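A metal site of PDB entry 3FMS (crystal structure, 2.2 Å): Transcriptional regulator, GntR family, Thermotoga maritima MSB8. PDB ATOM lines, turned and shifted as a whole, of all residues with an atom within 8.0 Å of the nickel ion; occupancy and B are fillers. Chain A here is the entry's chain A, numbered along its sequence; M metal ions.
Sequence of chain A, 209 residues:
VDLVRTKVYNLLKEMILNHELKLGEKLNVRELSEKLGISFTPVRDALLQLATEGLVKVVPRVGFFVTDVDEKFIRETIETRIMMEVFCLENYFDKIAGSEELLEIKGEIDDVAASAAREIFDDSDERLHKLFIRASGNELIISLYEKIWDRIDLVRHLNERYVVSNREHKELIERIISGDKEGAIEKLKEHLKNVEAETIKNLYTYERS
A ring nitrogen (NE2) of His 129 lies close to the side-chain carboxylate of Asp 125.
A ring nitrogen (ND1) of His 129 is in hydrogen-bond range of the guanidinium group (NH2) of Arg 81 (3.1 Å).
ND1 of His 129 sits at hydrogen-bond distance from OE1 of Glu 85, 2.5 Å away.
A ring nitrogen (ND1) of His 191 sits at hydrogen-bond distance from the side-chain carboxylate (OE1) of Glu 168, 2.7 Å away.
ND1 of His 169 sits close to O of Ser 165, at 3.4 Å.
The side-chain carboxylate (OD2) of Asp 125 lies within salt-bridge range of the guanidinium group (NH2) of Arg 156.
Merely in contact with the nickel ion: Asp 125 (3.0 Å).
Within 4 Å of the nickel ion: Asp 125, His 129, His 169 and His 191.
The nearest printed residue that does not touch the nickel ion is Arg 81 (4.7 Å).
The nickel ion is bound by NE2 of His 129, at 2.1 Å.
The nickel ion is bound by NE2 of His 191, at 2.1 Å.
NE2 of His 169 binds the nickel ion, at 2.1 Å.
The nickel ion has three donor atoms within binding distance.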
ATOM      1  N   ARG A  81      10.405  -7.991  -7.687  1.00  0.00           N
ATOM      2  CA  ARG A  81      11.663  -8.709  -7.552  1.00  0.00           C
ATOM      3  C   ARG A  81      12.813  -7.711  -7.525  1.00  0.00           C
ATOM      4  O   ARG A  81      13.752  -7.872  -6.738  1.00  0.00           O
ATOM      5  CB  ARG A  81      11.837  -9.633  -8.721  1.00  0.00           C
ATOM      6  CG  ARG A  81      10.924 -10.831  -8.677  1.00  0.00           C
ATOM      7  CD  ARG A  81      11.225 -11.755  -9.842  1.00  0.00           C
ATOM      8  NE  ARG A  81      12.557 -12.316  -9.768  1.00  0.00           N
ATOM      9  CZ  ARG A  81      13.124 -13.098 -10.675  1.00  0.00           C
ATOM     10  NH1 ARG A  81      12.501 -13.452 -11.768  1.00  0.00           N
ATOM     11  NH2 ARG A  81      14.366 -13.526 -10.463  1.00  0.00           N
ATOM     12  N   GLU A  85      15.264  -8.024  -4.453  1.00  0.00           N
ATOM     13  CA  GLU A  85      16.568  -8.571  -4.789  1.00  0.00           C
ATOM     14  C   GLU A  85      17.651  -7.501  -4.807  1.00  0.00           C
ATOM     15  O   GLU A  85      18.762  -7.724  -4.343  1.00  0.00           O
ATOM     16  CB  GLU A  85      16.530  -9.280  -6.121  1.00  0.00           C
ATOM     17  CG  GLU A  85      15.742 -10.551  -6.113  1.00  0.00           C
ATOM     18  CD  GLU A  85      15.757 -11.236  -7.472  1.00  0.00           C
ATOM     19  OE1 GLU A  85      16.805 -11.129  -8.142  1.00  0.00           O
ATOM     20  OE2 GLU A  85      14.798 -11.949  -7.810  1.00  0.00           O
ATOM     21  N   PHE A 121      19.465 -24.551 -16.302  1.00  0.00           N
ATOM     22  CA  PHE A 121      19.251 -23.113 -16.282  1.00  0.00           C
ATOM     23  C   PHE A 121      18.306 -22.796 -15.148  1.00  0.00           C
ATOM     24  O   PHE A 121      18.616 -21.972 -14.312  1.00  0.00           O
ATOM     25  CB  PHE A 121      18.768 -22.518 -17.644  1.00  0.00           C
ATOM     26  CG  PHE A 121      18.360 -21.121 -17.521  1.00  0.00           C
ATOM     27  CD1 PHE A 121      19.292 -20.105 -17.511  1.00  0.00           C
ATOM     28  CD2 PHE A 121      17.050 -20.815 -17.321  1.00  0.00           C
ATOM     29  CE1 PHE A 121      18.878 -18.769 -17.322  1.00  0.00           C
ATOM     30  CE2 PHE A 121      16.654 -19.504 -17.188  1.00  0.00           C
ATOM     31  CZ  PHE A 121      17.579 -18.486 -17.155  1.00  0.00           C
ATOM     32  N   SER A 124      19.997 -23.221 -11.724  1.00  0.00           N
ATOM     33  CA  SER A 124      20.977 -22.152 -11.469  1.00  0.00           C
ATOM     34  C   SER A 124      20.348 -20.749 -11.321  1.00  0.00           C
ATOM     35  O   SER A 124      20.774 -19.937 -10.468  1.00  0.00           O
ATOM     36  CB  SER A 124      21.989 -22.132 -12.606  1.00  0.00           C
ATOM     37  OG  SER A 124      21.481 -21.563 -13.823  1.00  0.00           O
ATOM     38  N   ASP A 125      19.364 -20.482 -12.161  1.00  0.00           N
ATOM     39  CA  ASP A 125      18.540 -19.251 -12.103  1.00  0.00           C
ATOM     40  C   ASP A 125      17.853 -19.040 -10.708  1.00  0.00           C
ATOM     41  O   ASP A 125      17.911 -17.967 -10.098  1.00  0.00           O
ATOM     42  CB  ASP A 125      17.468 -19.320 -13.206  1.00  0.00           C
ATOM     43  CG  ASP A 125      16.527 -18.103 -13.237  1.00  0.00           C
ATOM     44  OD1 ASP A 125      16.821 -17.059 -12.677  1.00  0.00           O
ATOM     45  OD2 ASP A 125      15.445 -18.242 -13.822  1.00  0.00           O
ATOM     46  N   GLU A 126      17.220 -20.086 -10.212  1.00  0.00           N
ATOM     47  CA  GLU A 126      16.549 -20.051  -8.919  1.00  0.00           C
ATOM     48  C   GLU A 126      17.550 -19.858  -7.810  1.00  0.00           C
ATOM     49  O   GLU A 126      17.329 -19.093  -6.882  1.00  0.00           O
ATOM     50  CB  GLU A 126      15.790 -21.362  -8.730  1.00  0.00           C
ATOM     51  CG  GLU A 126      15.344 -21.666  -7.326  1.00  0.00           C
ATOM     52  CD  GLU A 126      14.261 -22.804  -7.243  1.00  0.00           C
ATOM     53  OE1 GLU A 126      14.109 -23.634  -8.168  1.00  0.00           O
ATOM     54  OE2 GLU A 126      13.565 -22.847  -6.233  1.00  0.00           O
ATOM     55  N   LEU A 128      20.531 -18.495  -7.813  1.00  0.00           N
ATOM     56  CA  LEU A 128      21.224 -17.232  -7.791  1.00  0.00           C
ATOM     57  C   LEU A 128      20.345 -16.177  -7.218  1.00  0.00           C
ATOM     58  O   LEU A 128      20.786 -15.368  -6.411  1.00  0.00           O
ATOM     59  CB  LEU A 128      21.609 -16.789  -9.161  1.00  0.00           C
ATOM     60  CG  LEU A 128      22.344 -15.441  -9.240  1.00  0.00           C
ATOM     61  CD1 LEU A 128      23.672 -15.507  -8.535  1.00  0.00           C
ATOM     62  CD2 LEU A 128      22.549 -15.120 -10.687  1.00  0.00           C
ATOM     63  N   HIS A 129      19.118 -16.112  -7.714  1.00  0.00           N
ATOM     64  CA  HIS A 129      18.209 -15.048  -7.289  1.00  0.00           C
ATOM     65  C   HIS A 129      17.834 -15.253  -5.816  1.00  0.00           C
ATOM     66  O   HIS A 129      17.849 -14.318  -5.051  1.00  0.00           O
ATOM     67  CB  HIS A 129      16.980 -14.968  -8.161  1.00  0.00           C
ATOM     68  CG  HIS A 129      17.231 -14.375  -9.517  1.00  0.00           C
ATOM     69  ND1 HIS A 129      17.304 -13.029  -9.728  1.00  0.00           N
ATOM     70  CD2 HIS A 129      17.401 -14.947 -10.729  1.00  0.00           C
ATOM     71  CE1 HIS A 129      17.560 -12.785 -10.988  1.00  0.00           C
ATOM     72  NE2 HIS A 129      17.606 -13.936 -11.627  1.00  0.00           N
ATOM     73  N   PHE A 132      20.540 -14.144  -3.203  1.00  0.00           N
ATOM     74  CA  PHE A 132      20.479 -12.722  -2.821  1.00  0.00           C
ATOM     75  C   PHE A 132      19.546 -12.538  -1.642  1.00  0.00           C
ATOM     76  O   PHE A 132      19.917 -11.964  -0.648  1.00  0.00           O
ATOM     77  CB  PHE A 132      20.030 -11.862  -3.983  1.00  0.00           C
ATOM     78  CG  PHE A 132      20.879 -11.974  -5.212  1.00  0.00           C
ATOM     79  CD1 PHE A 132      22.244 -12.324  -5.124  1.00  0.00           C
ATOM     80  CD2 PHE A 132      20.355 -11.737  -6.432  1.00  0.00           C
ATOM     81  CE1 PHE A 132      23.005 -12.440  -6.253  1.00  0.00           C
ATOM     82  CE2 PHE A 132      21.131 -11.834  -7.586  1.00  0.00           C
ATOM     83  CZ  PHE A 132      22.472 -12.182  -7.481  1.00  0.00           C
ATOM     84  N   ARG A 156       8.923 -16.499 -14.866  1.00  0.00           N
ATOM     85  CA  ARG A 156      10.259 -16.924 -15.394  1.00  0.00           C
ATOM     86  C   ARG A 156      10.109 -17.744 -16.656  1.00  0.00           C
ATOM     87  O   ARG A 156      10.961 -17.745 -17.534  1.00  0.00           O
ATOM     88  CB  ARG A 156      10.988 -17.969 -14.488  1.00  0.00           C
ATOM     89  CG  ARG A 156      11.515 -17.561 -13.284  1.00  0.00           C
ATOM     90  CD  ARG A 156      12.623 -18.594 -12.839  1.00  0.00           C
ATOM     91  NE  ARG A 156      12.225 -19.941 -12.309  1.00  0.00           N
ATOM     92  CZ  ARG A 156      13.127 -20.910 -12.045  1.00  0.00           C
ATOM     93  NH1 ARG A 156      12.800 -22.113 -11.532  1.00  0.00           N
ATOM     94  NH2 ARG A 156      14.395 -20.676 -12.264  1.00  0.00           N
ATOM     95  N   ARG A 161      14.134 -16.963 -23.800  1.00  0.00           N
ATOM     96  CA  ARG A 161      15.517 -16.531 -24.051  1.00  0.00           C
ATOM     97  C   ARG A 161      16.461 -16.850 -22.894  1.00  0.00           C
ATOM     98  O   ARG A 161      17.240 -16.008 -22.443  1.00  0.00           O
ATOM     99  CB  ARG A 161      15.573 -15.036 -24.399  1.00  0.00           C
ATOM    100  CG  ARG A 161      14.833 -14.122 -23.434  1.00  0.00           C
ATOM    101  CD  ARG A 161      15.525 -12.764 -23.364  1.00  0.00           C
ATOM    102  NE  ARG A 161      16.186 -12.671 -22.084  1.00  0.00           N
ATOM    103  CZ  ARG A 161      17.116 -11.777 -21.712  1.00  0.00           C
ATOM    104  NH1 ARG A 161      17.575 -10.774 -22.499  1.00  0.00           N
ATOM    105  NH2 ARG A 161      17.577 -11.903 -20.457  1.00  0.00           N
ATOM    106  N   SER A 165      19.685 -14.971 -20.867  1.00  0.00           N
ATOM    107  CA  SER A 165      19.600 -14.808 -19.403  1.00  0.00           C
ATOM    108  C   SER A 165      20.734 -15.488 -18.709  1.00  0.00           C
ATOM    109  O   SER A 165      21.278 -14.960 -17.744  1.00  0.00           O
ATOM    110  CB  SER A 165      18.292 -15.370 -18.876  1.00  0.00           C
ATOM    111  OG  SER A 165      17.207 -14.611 -19.379  1.00  0.00           O
ATOM    112  N   ASN A 166      21.129 -16.636 -19.224  1.00  0.00           N
ATOM    113  CA  ASN A 166      22.284 -17.282 -18.663  1.00  0.00           C
ATOM    114  C   ASN A 166      23.513 -16.407 -18.738  1.00  0.00           C
ATOM    115  O   ASN A 166      24.301 -16.369 -17.809  1.00  0.00           O
ATOM    116  CB  ASN A 166      22.513 -18.648 -19.307  1.00  0.00           C
ATOM    117  CG  ASN A 166      23.551 -19.485 -18.577  1.00  0.00           C
ATOM    118  OD1 ASN A 166      23.366 -19.979 -17.413  1.00  0.00           O
ATOM    119  ND2 ASN A 166      24.675 -19.636 -19.230  1.00  0.00           N
ATOM    120  N   GLU A 168      23.645 -13.079 -18.961  1.00  0.00           N
ATOM    121  CA  GLU A 168      23.456 -12.016 -17.992  1.00  0.00           C
ATOM    122  C   GLU A 168      23.752 -12.406 -16.540  1.00  0.00           C
ATOM    123  O   GLU A 168      24.299 -11.633 -15.764  1.00  0.00           O
ATOM    124  CB  GLU A 168      22.053 -11.439 -18.109  1.00  0.00           C
ATOM    125  CG  GLU A 168      21.782 -10.755 -19.476  1.00  0.00           C
ATOM    126  CD  GLU A 168      20.319 -10.416 -19.711  1.00  0.00           C
ATOM    127  OE1 GLU A 168      19.470 -10.785 -18.840  1.00  0.00           O
ATOM    128  OE2 GLU A 168      20.006  -9.812 -20.758  1.00  0.00           O
ATOM    129  N   HIS A 169      23.324 -13.588 -16.143  1.00  0.00           N
ATOM    130  CA  HIS A 169      23.693 -14.046 -14.825  1.00  0.00           C
ATOM    131  C   HIS A 169      25.217 -14.133 -14.712  1.00  0.00           C
ATOM    132  O   HIS A 169      25.772 -13.794 -13.692  1.00  0.00           O
ATOM    133  CB  HIS A 169      23.153 -15.442 -14.553  1.00  0.00           C
ATOM    134  CG  HIS A 169      21.667 -15.532 -14.503  1.00  0.00           C
ATOM    135  ND1 HIS A 169      21.012 -16.699 -14.811  1.00  0.00           N
ATOM    136  CD2 HIS A 169      20.713 -14.634 -14.162  1.00  0.00           C
ATOM    137  CE1 HIS A 169      19.725 -16.519 -14.676  1.00  0.00           C
ATOM    138  NE2 HIS A 169      19.511 -15.273 -14.272  1.00  0.00           N
ATOM    139  N   LEU A 172      26.716 -10.871 -14.074  1.00  0.00           N
ATOM    140  CA  LEU A 172      26.366 -10.439 -12.738  1.00  0.00           C
ATOM    141  C   LEU A 172      27.311 -10.993 -11.719  1.00  0.00           C
ATOM    142  O   LEU A 172      27.794 -10.330 -10.815  1.00  0.00           O
ATOM    143  CB  LEU A 172      24.986 -11.020 -12.346  1.00  0.00           C
ATOM    144  CG  LEU A 172      23.934 -10.176 -11.659  1.00  0.00           C
ATOM    145  CD1 LEU A 172      22.682 -10.968 -11.140  1.00  0.00           C
ATOM    146  CD2 LEU A 172      24.512  -9.290 -10.615  1.00  0.00           C
ATOM    147  N   LEU A 188      21.893  -6.300 -12.358  1.00  0.00           N
ATOM    148  CA  LEU A 188      20.691  -7.063 -11.897  1.00  0.00           C
ATOM    149  C   LEU A 188      19.432  -6.350 -12.377  1.00  0.00           C
ATOM    150  O   LEU A 188      18.533  -6.971 -12.905  1.00  0.00           O
ATOM    151  CB  LEU A 188      20.646  -7.275 -10.389  1.00  0.00           C
ATOM    152  CG  LEU A 188      19.431  -7.965  -9.771  1.00  0.00           C
ATOM    153  CD1 LEU A 188      19.007  -9.298 -10.426  1.00  0.00           C
ATOM    154  CD2 LEU A 188      19.753  -8.076  -8.389  1.00  0.00           C
ATOM    155  N   HIS A 191      19.212  -6.918 -16.076  1.00  0.00           N
ATOM    156  CA  HIS A 191      18.797  -8.281 -16.377  1.00  0.00           C
ATOM    157  C   HIS A 191      17.286  -8.484 -16.210  1.00  0.00           C
ATOM    158  O   HIS A 191      16.615  -8.986 -17.063  1.00  0.00           O
ATOM    159  CB  HIS A 191      19.569  -9.186 -15.458  1.00  0.00           C
ATOM    160  CG  HIS A 191      18.995 -10.564 -15.281  1.00  0.00           C
ATOM    161  ND1 HIS A 191      18.789 -11.427 -16.325  1.00  0.00           N
ATOM    162  CD2 HIS A 191      18.692 -11.259 -14.146  1.00  0.00           C
ATOM    163  CE1 HIS A 191      18.340 -12.576 -15.860  1.00  0.00           C
ATOM    164  NE2 HIS A 191      18.244 -12.498 -14.536  1.00  0.00           N
ATOM    165  N   LEU A 192      16.760  -8.042 -15.114  1.00  0.00           N
ATOM    166  CA  LEU A 192      15.343  -8.202 -14.842  1.00  0.00           C
ATOM    167  C   LEU A 192      14.456  -7.397 -15.753  1.00  0.00           C
ATOM    168  O   LEU A 192      13.415  -7.884 -16.169  1.00  0.00           O
ATOM    169  CB  LEU A 192      15.067  -7.866 -13.389  1.00  0.00           C
ATOM    170  CG  LEU A 192      15.553  -8.959 -12.417  1.00  0.00           C
ATOM    171  CD1 LEU A 192      15.474  -8.425 -11.043  1.00  0.00           C
ATOM    172  CD2 LEU A 192      14.846 -10.262 -12.548  1.00  0.00           C
ATOM    173  N   VAL A 195      14.586  -9.261 -19.100  1.00  0.00           N
ATOM    174  CA  VAL A 195      13.663 -10.391 -18.983  1.00  0.00           C
ATOM    175  C   VAL A 195      12.167  -9.922 -19.087  1.00  0.00           C
ATOM    176  O   VAL A 195      11.375 -10.482 -19.838  1.00  0.00           O
ATOM    177  CB  VAL A 195      13.943 -11.157 -17.689  1.00  0.00           C
ATOM    178  CG1 VAL A 195      12.881 -12.122 -17.409  1.00  0.00           C
ATOM    179  CG2 VAL A 195      15.292 -11.878 -17.791  1.00  0.00           C
HETATM  180 NI    NI M   1      17.709 -14.330 -13.663  1.00  0.00          NI
